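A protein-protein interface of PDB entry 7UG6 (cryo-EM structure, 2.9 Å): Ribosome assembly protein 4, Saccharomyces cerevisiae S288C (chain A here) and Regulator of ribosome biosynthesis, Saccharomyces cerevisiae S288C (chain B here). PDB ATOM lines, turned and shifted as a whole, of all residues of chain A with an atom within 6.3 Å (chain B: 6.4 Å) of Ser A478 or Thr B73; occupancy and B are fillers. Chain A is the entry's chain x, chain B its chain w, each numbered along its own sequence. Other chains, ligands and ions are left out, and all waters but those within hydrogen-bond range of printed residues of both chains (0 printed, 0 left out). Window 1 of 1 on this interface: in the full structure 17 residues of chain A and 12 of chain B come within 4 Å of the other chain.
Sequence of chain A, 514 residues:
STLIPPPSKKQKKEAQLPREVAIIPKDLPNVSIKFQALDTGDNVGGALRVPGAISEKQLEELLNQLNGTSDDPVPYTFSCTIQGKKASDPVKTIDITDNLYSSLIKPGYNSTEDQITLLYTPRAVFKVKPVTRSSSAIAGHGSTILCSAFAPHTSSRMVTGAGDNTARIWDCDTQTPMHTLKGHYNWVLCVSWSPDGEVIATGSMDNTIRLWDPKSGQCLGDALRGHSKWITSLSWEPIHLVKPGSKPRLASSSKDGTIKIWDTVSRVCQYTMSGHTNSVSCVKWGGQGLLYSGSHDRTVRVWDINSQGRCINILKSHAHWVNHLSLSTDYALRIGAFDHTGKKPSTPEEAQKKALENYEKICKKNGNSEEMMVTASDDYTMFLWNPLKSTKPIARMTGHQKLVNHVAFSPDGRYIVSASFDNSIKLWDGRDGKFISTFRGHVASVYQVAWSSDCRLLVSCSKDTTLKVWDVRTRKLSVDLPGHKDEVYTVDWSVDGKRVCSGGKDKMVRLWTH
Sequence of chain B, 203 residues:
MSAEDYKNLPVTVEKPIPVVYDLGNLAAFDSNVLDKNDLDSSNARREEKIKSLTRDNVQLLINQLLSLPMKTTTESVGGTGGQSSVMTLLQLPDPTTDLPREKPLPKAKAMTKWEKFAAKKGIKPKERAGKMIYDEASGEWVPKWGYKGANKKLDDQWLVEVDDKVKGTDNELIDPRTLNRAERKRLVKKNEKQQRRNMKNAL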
ATOM      1  N   PRO A 130      -6.343  18.899  11.859  1.00  0.00           N
ATOM      2  CA  PRO A 130      -6.993  19.353  13.093  1.00  0.00           C
ATOM      3  C   PRO A 130      -8.289  18.611  13.350  1.00  0.00           C
ATOM      4  O   PRO A 130      -9.031  18.273  12.432  1.00  0.00           O
ATOM      5  CB  PRO A 130      -7.252  20.839  12.836  1.00  0.00           C
ATOM      6  CG  PRO A 130      -6.318  21.205  11.756  1.00  0.00           C
ATOM      7  CD  PRO A 130      -6.158  19.997  10.901  1.00  0.00           C
ATOM      8  N   LEU A 457      -0.269  21.587  16.906  1.00  0.00           N
ATOM      9  CA  LEU A 457      -1.617  21.763  17.413  1.00  0.00           C
ATOM     10  C   LEU A 457      -1.675  21.389  18.880  1.00  0.00           C
ATOM     11  O   LEU A 457      -1.017  20.449  19.324  1.00  0.00           O
ATOM     12  CB  LEU A 457      -2.611  20.907  16.635  1.00  0.00           C
ATOM     13  CG  LEU A 457      -2.887  21.329  15.199  1.00  0.00           C
ATOM     14  CD1 LEU A 457      -3.548  20.215  14.451  1.00  0.00           C
ATOM     15  CD2 LEU A 457      -3.771  22.542  15.194  1.00  0.00           C
ATOM     16  N   VAL A 469      -8.957  23.458  20.223  1.00  0.00           N
ATOM     17  CA  VAL A 469      -7.655  23.180  19.641  1.00  0.00           C
ATOM     18  C   VAL A 469      -7.075  24.498  19.168  1.00  0.00           C
ATOM     19  O   VAL A 469      -7.799  25.429  18.808  1.00  0.00           O
ATOM     20  CB  VAL A 469      -7.689  22.171  18.477  1.00  0.00           C
ATOM     21  CG1 VAL A 469      -8.220  20.832  18.935  1.00  0.00           C
ATOM     22  CG2 VAL A 469      -8.428  22.703  17.342  1.00  0.00           C
ATOM     23  N   TRP A 470      -5.758  24.577  19.172  1.00  0.00           N
ATOM     24  CA  TRP A 470      -5.075  25.835  18.951  1.00  0.00           C
ATOM     25  C   TRP A 470      -4.011  25.662  17.888  1.00  0.00           C
ATOM     26  O   TRP A 470      -3.289  24.665  17.877  1.00  0.00           O
ATOM     27  CB  TRP A 470      -4.454  26.332  20.240  1.00  0.00           C
ATOM     28  CG  TRP A 470      -5.384  26.273  21.386  1.00  0.00           C
ATOM     29  CD1 TRP A 470      -5.620  25.213  22.188  1.00  0.00           C
ATOM     30  CD2 TRP A 470      -6.218  27.324  21.852  1.00  0.00           C
ATOM     31  NE1 TRP A 470      -6.547  25.535  23.136  1.00  0.00           N
ATOM     32  CE2 TRP A 470      -6.933  26.831  22.946  1.00  0.00           C
ATOM     33  CE3 TRP A 470      -6.427  28.639  21.450  1.00  0.00           C
ATOM     34  CZ2 TRP A 470      -7.837  27.597  23.639  1.00  0.00           C
ATOM     35  CZ3 TRP A 470      -7.313  29.395  22.136  1.00  0.00           C
ATOM     36  CH2 TRP A 470      -8.017  28.876  23.219  1.00  0.00           C
ATOM     37  N   ASP A 471      -3.919  26.636  16.996  1.00  0.00           N
ATOM     38  CA  ASP A 471      -2.892  26.644  15.969  1.00  0.00           C
ATOM     39  C   ASP A 471      -1.674  27.354  16.534  1.00  0.00           C
ATOM     40  O   ASP A 471      -1.708  28.566  16.756  1.00  0.00           O
ATOM     41  CB  ASP A 471      -3.386  27.346  14.710  1.00  0.00           C
ATOM     42  CG  ASP A 471      -2.537  27.037  13.503  1.00  0.00           C
ATOM     43  OD1 ASP A 471      -1.672  26.146  13.600  1.00  0.00           O
ATOM     44  OD2 ASP A 471      -2.725  27.689  12.458  1.00  0.00           O
ATOM     45  N   LYS A 476      -3.606  31.106  17.593  1.00  0.00           N
ATOM     46  CA  LYS A 476      -5.021  31.436  17.565  1.00  0.00           C
ATOM     47  C   LYS A 476      -5.831  30.162  17.723  1.00  0.00           C
ATOM     48  O   LYS A 476      -5.347  29.063  17.460  1.00  0.00           O
ATOM     49  CB  LYS A 476      -5.387  32.157  16.261  1.00  0.00           C
ATOM     50  CG  LYS A 476      -6.750  32.814  16.242  1.00  0.00           C
ATOM     51  CD  LYS A 476      -6.947  33.657  15.003  1.00  0.00           C
ATOM     52  CE  LYS A 476      -7.198  32.792  13.789  1.00  0.00           C
ATOM     53  NZ  LYS A 476      -7.503  33.606  12.576  1.00  0.00           N
ATOM     54  N   LEU A 477      -7.068  30.323  18.173  1.00  0.00           N
ATOM     55  CA  LEU A 477      -7.992  29.204  18.235  1.00  0.00           C
ATOM     56  C   LEU A 477      -8.244  28.659  16.840  1.00  0.00           C
ATOM     57  O   LEU A 477      -8.277  29.406  15.863  1.00  0.00           O
ATOM     58  CB  LEU A 477      -9.305  29.645  18.871  1.00  0.00           C
ATOM     59  CG  LEU A 477     -10.315  28.563  19.203  1.00  0.00           C
ATOM     60  CD1 LEU A 477      -9.741  27.654  20.221  1.00  0.00           C
ATOM     61  CD2 LEU A 477     -11.564  29.181  19.746  1.00  0.00           C
ATOM     62  N   SER A 478      -8.398  27.343  16.743  1.00  0.00           N
ATOM     63  CA  SER A 478      -8.715  26.705  15.474  1.00  0.00           C
ATOM     64  C   SER A 478     -10.162  26.231  15.430  1.00  0.00           C
ATOM     65  O   SER A 478     -10.918  26.638  14.544  1.00  0.00           O
ATOM     66  CB  SER A 478      -7.752  25.548  15.217  1.00  0.00           C
ATOM     67  OG  SER A 478      -8.149  24.801  14.087  1.00  0.00           O
ATOM     68  N   VAL A 479     -10.574  25.391  16.373  1.00  0.00           N
ATOM     69  CA  VAL A 479     -11.985  25.040  16.491  1.00  0.00           C
ATOM     70  C   VAL A 479     -12.346  24.900  17.961  1.00  0.00           C
ATOM     71  O   VAL A 479     -11.587  24.331  18.748  1.00  0.00           O
ATOM     72  CB  VAL A 479     -12.349  23.765  15.699  1.00  0.00           C
ATOM     73  CG1 VAL A 479     -11.649  22.574  16.213  1.00  0.00           C
ATOM     74  CG2 VAL A 479     -13.829  23.504  15.784  1.00  0.00           C
ATOM     75  N   ASP A 480     -13.485  25.469  18.339  1.00  0.00           N
ATOM     76  CA  ASP A 480     -14.099  25.167  19.616  1.00  0.00           C
ATOM     77  C   ASP A 480     -14.892  23.882  19.494  1.00  0.00           C
ATOM     78  O   ASP A 480     -15.562  23.640  18.490  1.00  0.00           O
ATOM     79  CB  ASP A 480     -15.018  26.296  20.062  1.00  0.00           C
ATOM     80  CG  ASP A 480     -15.604  26.057  21.443  1.00  0.00           C
ATOM     81  OD1 ASP A 480     -16.581  26.745  21.803  1.00  0.00           O
ATOM     82  OD2 ASP A 480     -15.085  25.183  22.172  1.00  0.00           O
ATOM     83  N   LYS B  71     -13.866  35.362   5.614  1.00  0.00           N
ATOM     84  CA  LYS B  71     -14.030  35.080   7.022  1.00  0.00           C
ATOM     85  C   LYS B  71     -13.863  33.595   7.250  1.00  0.00           C
ATOM     86  O   LYS B  71     -14.216  32.772   6.405  1.00  0.00           O
ATOM     87  CB  LYS B  71     -15.387  35.540   7.562  1.00  0.00           C
ATOM     88  CG  LYS B  71     -16.541  34.616   7.283  1.00  0.00           C
ATOM     89  CD  LYS B  71     -17.797  35.141   7.929  1.00  0.00           C
ATOM     90  CE  LYS B  71     -17.649  35.191   9.434  1.00  0.00           C
ATOM     91  NZ  LYS B  71     -17.500  33.841  10.025  1.00  0.00           N
ATOM     92  N   THR B  72     -13.284  33.266   8.390  1.00  0.00           N
ATOM     93  CA  THR B  72     -13.155  31.884   8.802  1.00  0.00           C
ATOM     94  C   THR B  72     -13.592  31.788  10.249  1.00  0.00           C
ATOM     95  O   THR B  72     -13.409  32.728  11.026  1.00  0.00           O
ATOM     96  CB  THR B  72     -11.725  31.377   8.607  1.00  0.00           C
ATOM     97  OG1 THR B  72     -11.678  29.971   8.869  1.00  0.00           O
ATOM     98  CG2 THR B  72     -10.749  32.116   9.506  1.00  0.00           C
ATOM     99  N   THR B  73     -14.208  30.673  10.596  1.00  0.00           N
ATOM    100  CA  THR B  73     -14.810  30.551  11.905  1.00  0.00           C
ATOM    101  C   THR B  73     -14.093  29.480  12.711  1.00  0.00           C
ATOM    102  O   THR B  73     -13.185  28.805  12.231  1.00  0.00           O
ATOM    103  CB  THR B  73     -16.291  30.236  11.774  1.00  0.00           C
ATOM    104  OG1 THR B  73     -16.899  30.290  13.064  1.00  0.00           O
ATOM    105  CG2 THR B  73     -16.473  28.860  11.220  1.00  0.00           C
ATOM    106  N   THR B  74     -14.505  29.328  13.960  1.00  0.00           N
ATOM    107  CA  THR B  74     -13.989  28.282  14.816  1.00  0.00           C
ATOM    108  C   THR B  74     -15.080  27.351  15.307  1.00  0.00           C
ATOM    109  O   THR B  74     -14.866  26.628  16.282  1.00  0.00           O
ATOM    110  CB  THR B  74     -13.256  28.886  16.013  1.00  0.00           C
ATOM    111  OG1 THR B  74     -14.193  29.577  16.842  1.00  0.00           O
ATOM    112  CG2 THR B  74     -12.191  29.854  15.546  1.00  0.00           C
ATOM    113  N   GLU B  75     -16.242  27.360  14.673  1.00  0.00           N
ATOM    114  CA  GLU B  75     -17.360  26.539  15.101  1.00  0.00           C
ATOM    115  C   GLU B  75     -17.203  25.101  14.618  1.00  0.00           C
ATOM    116  O   GLU B  75     -16.749  24.842  13.506  1.00  0.00           O
ATOM    117  CB  GLU B  75     -18.656  27.141  14.574  1.00  0.00           C
ATOM    118  CG  GLU B  75     -19.925  26.441  14.998  1.00  0.00           C
ATOM    119  CD  GLU B  75     -21.158  27.145  14.468  1.00  0.00           C
ATOM    120  OE1 GLU B  75     -21.002  28.161  13.759  1.00  0.00           O
ATOM    121  OE2 GLU B  75     -22.281  26.680  14.741  1.00  0.00           O
ATOM    122  N   GLN B  83     -21.183  27.840   8.814  1.00  0.00           N
ATOM    123  CA  GLN B  83     -20.011  27.194   8.267  1.00  0.00           C
ATOM    124  C   GLN B  83     -19.237  26.487   9.366  1.00  0.00           C
ATOM    125  O   GLN B  83     -19.314  26.842  10.541  1.00  0.00           O
ATOM    126  CB  GLN B  83     -19.100  28.207   7.587  1.00  0.00           C
ATOM    127  CG  GLN B  83     -18.834  29.426   8.415  1.00  0.00           C
ATOM    128  CD  GLN B  83     -17.712  30.249   7.850  1.00  0.00           C
ATOM    129  OE1 GLN B  83     -17.814  31.465   7.754  1.00  0.00           O
ATOM    130  NE2 GLN B  83     -16.633  29.592   7.461  1.00  0.00           N
ATOM    131  N   SER B  84     -18.476  25.480   8.968  1.00  0.00           N
ATOM    132  CA  SER B  84     -17.623  24.744   9.881  1.00  0.00           C
ATOM    133  C   SER B  84     -16.277  25.441  10.006  1.00  0.00           C
ATOM    134  O   SER B  84     -15.940  26.335   9.231  1.00  0.00           O
ATOM    135  CB  SER B  84     -17.434  23.305   9.404  1.00  0.00           C
ATOM    136  OG  SER B  84     -16.385  22.679  10.117  1.00  0.00           O
ATOM    137  N   SER B  85     -15.507  25.016  11.004  1.00  0.00           N
ATOM    138  CA  SER B  85     -14.262  25.700  11.337  1.00  0.00           C
ATOM    139  C   SER B  85     -13.235  25.596  10.230  1.00  0.00           C
ATOM    140  O   SER B  85     -12.342  26.441  10.125  1.00  0.00           O
ATOM    141  CB  SER B  85     -13.685  25.109  12.611  1.00  0.00           C
ATOM    142  OG  SER B  85     -13.716  23.695  12.536  1.00  0.00           O
ATOM    143  N   VAL B  86     -13.339  24.560   9.404  1.00  0.00           N
ATOM    144  CA  VAL B  86     -12.287  24.242   8.461  1.00  0.00           C
ATOM    145  C   VAL B  86     -12.374  25.087   7.202  1.00  0.00           C
ATOM    146  O   VAL B  86     -11.342  25.442   6.625  1.00  0.00           O
ATOM    147  CB  VAL B  86     -12.365  22.738   8.164  1.00  0.00           C
ATOM    148  CG1 VAL B  86     -13.738  22.408   7.632  1.00  0.00           C
ATOM    149  CG2 VAL B  86     -11.273  22.329   7.201  1.00  0.00           C
ATOM    150  N   MET B  87     -13.575  25.458   6.781  1.00  0.00           N
ATOM    151  CA  MET B  87     -13.783  26.086   5.492  1.00  0.00           C
ATOM    152  C   MET B  87     -13.831  27.598   5.627  1.00  0.00           C
ATOM    153  O   MET B  87     -14.546  28.140   6.472  1.00  0.00           O
ATOM    154  CB  MET B  87     -15.046  25.537   4.834  1.00  0.00           C
ATOM    155  CG  MET B  87     -16.368  25.814   5.501  1.00  0.00           C
ATOM    156  SD  MET B  87     -17.608  24.982   4.503  1.00  0.00           S
ATOM    157  CE  MET B  87     -19.099  25.353   5.377  1.00  0.00           C
ATOM    158  N   THR B  88     -13.038  28.268   4.800  1.00  0.00           N
ATOM    159  CA  THR B  88     -12.924  29.716   4.807  1.00  0.00           C
ATOM    160  C   THR B  88     -13.778  30.283   3.688  1.00  0.00           C
ATOM    161  O   THR B  88     -13.529  30.004   2.516  1.00  0.00           O
ATOM    162  CB  THR B  88     -11.477  30.150   4.624  1.00  0.00           C
ATOM    163  OG1 THR B  88     -10.711  29.746   5.762  1.00  0.00           O
ATOM    164  CG2 THR B  88     -11.407  31.640   4.489  1.00  0.00           C
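The backbone carbonyl oxygen (O) of Thr B74 is in hydrogen-bond range of the backbone NH (N) of Asp A480 (2.7 Å).
The backbone NH (N) of Glu B75 sits at hydrogen-bond distance from the side-chain hydroxyl (OG1) of Thr B73, 3.4 Å away.
The backbone NH (N) of Ser B85 sits at hydrogen-bond distance from the backbone carbonyl oxygen (O) of Glu B75.
The backbone NH of Ser A478 lies within hydrogen-bond range of the backbone carbonyl oxygen of Val A469.
The backbone NH (N) of Val A469 is in hydrogen-bond range of the backbone carbonyl oxygen (O) of Val A479, at 3.1 Å.
Among the printed residues, pairs that only touch across the chains: Val A479 with Ser B85 (3.3 Å), Val A479 with Thr B74 (3.3 Å), Ser A478 with Thr B74 (3.5 Å), Ser A478 with Ser B85 (3.7 Å), Ser A478 with Thr B73 (3.9 Å), Val A479 with Glu B75 (3.9 Å) and Leu A477 with Thr B74 (3.9 Å).
Of the printed residues of chain B, Leu A477 touches Thr B74.
Ser A478 touches just these residues of chain B: Thr B73 (3.9 Å), Thr B74 (3.5 Å) and Ser B85 (3.7 Å).
Printed residues of chain B within 4 Å of Val A479: Thr B74, Glu B75 and Ser B85.
Of the printed residues of chain A, Thr B74 touches Leu A477 (3.9 Å), Ser A478 (3.5 Å), Val A479 (3.3 Å) and Asp A480 (2.7 Å).
Printed residues of chain A within 4 Å of Glu B75: Val A479.
Printed residues of chain A within 4 Å of Ser B85: Ser A478 and Val A479.
The nearest residue of chain B that does not touch Ser A478 is Glu B75 (5.4 Å).
The nearest printed residue of chain B that does not touch Val A479 is Thr B73 (5.8 Å).
Of the 11 printed residues of chain B, 4 touch a printed residue of chain A.
Printed residues of chain B that touch a printed residue of chain A: Thr B73, Thr B74, Glu B75 and Ser B85.
Along chain B the printed residues that touch a printed residue of chain A span positions 73 to 85.
Hydrophobic or aromatic side chains of chain A that line the printed part of chain B: Leu A477 and Val A479.
Among the printed residues, no Asp or Glu carboxylate lies within 4 Å of a Lys or Arg side-chain nitrogen of the other chain.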
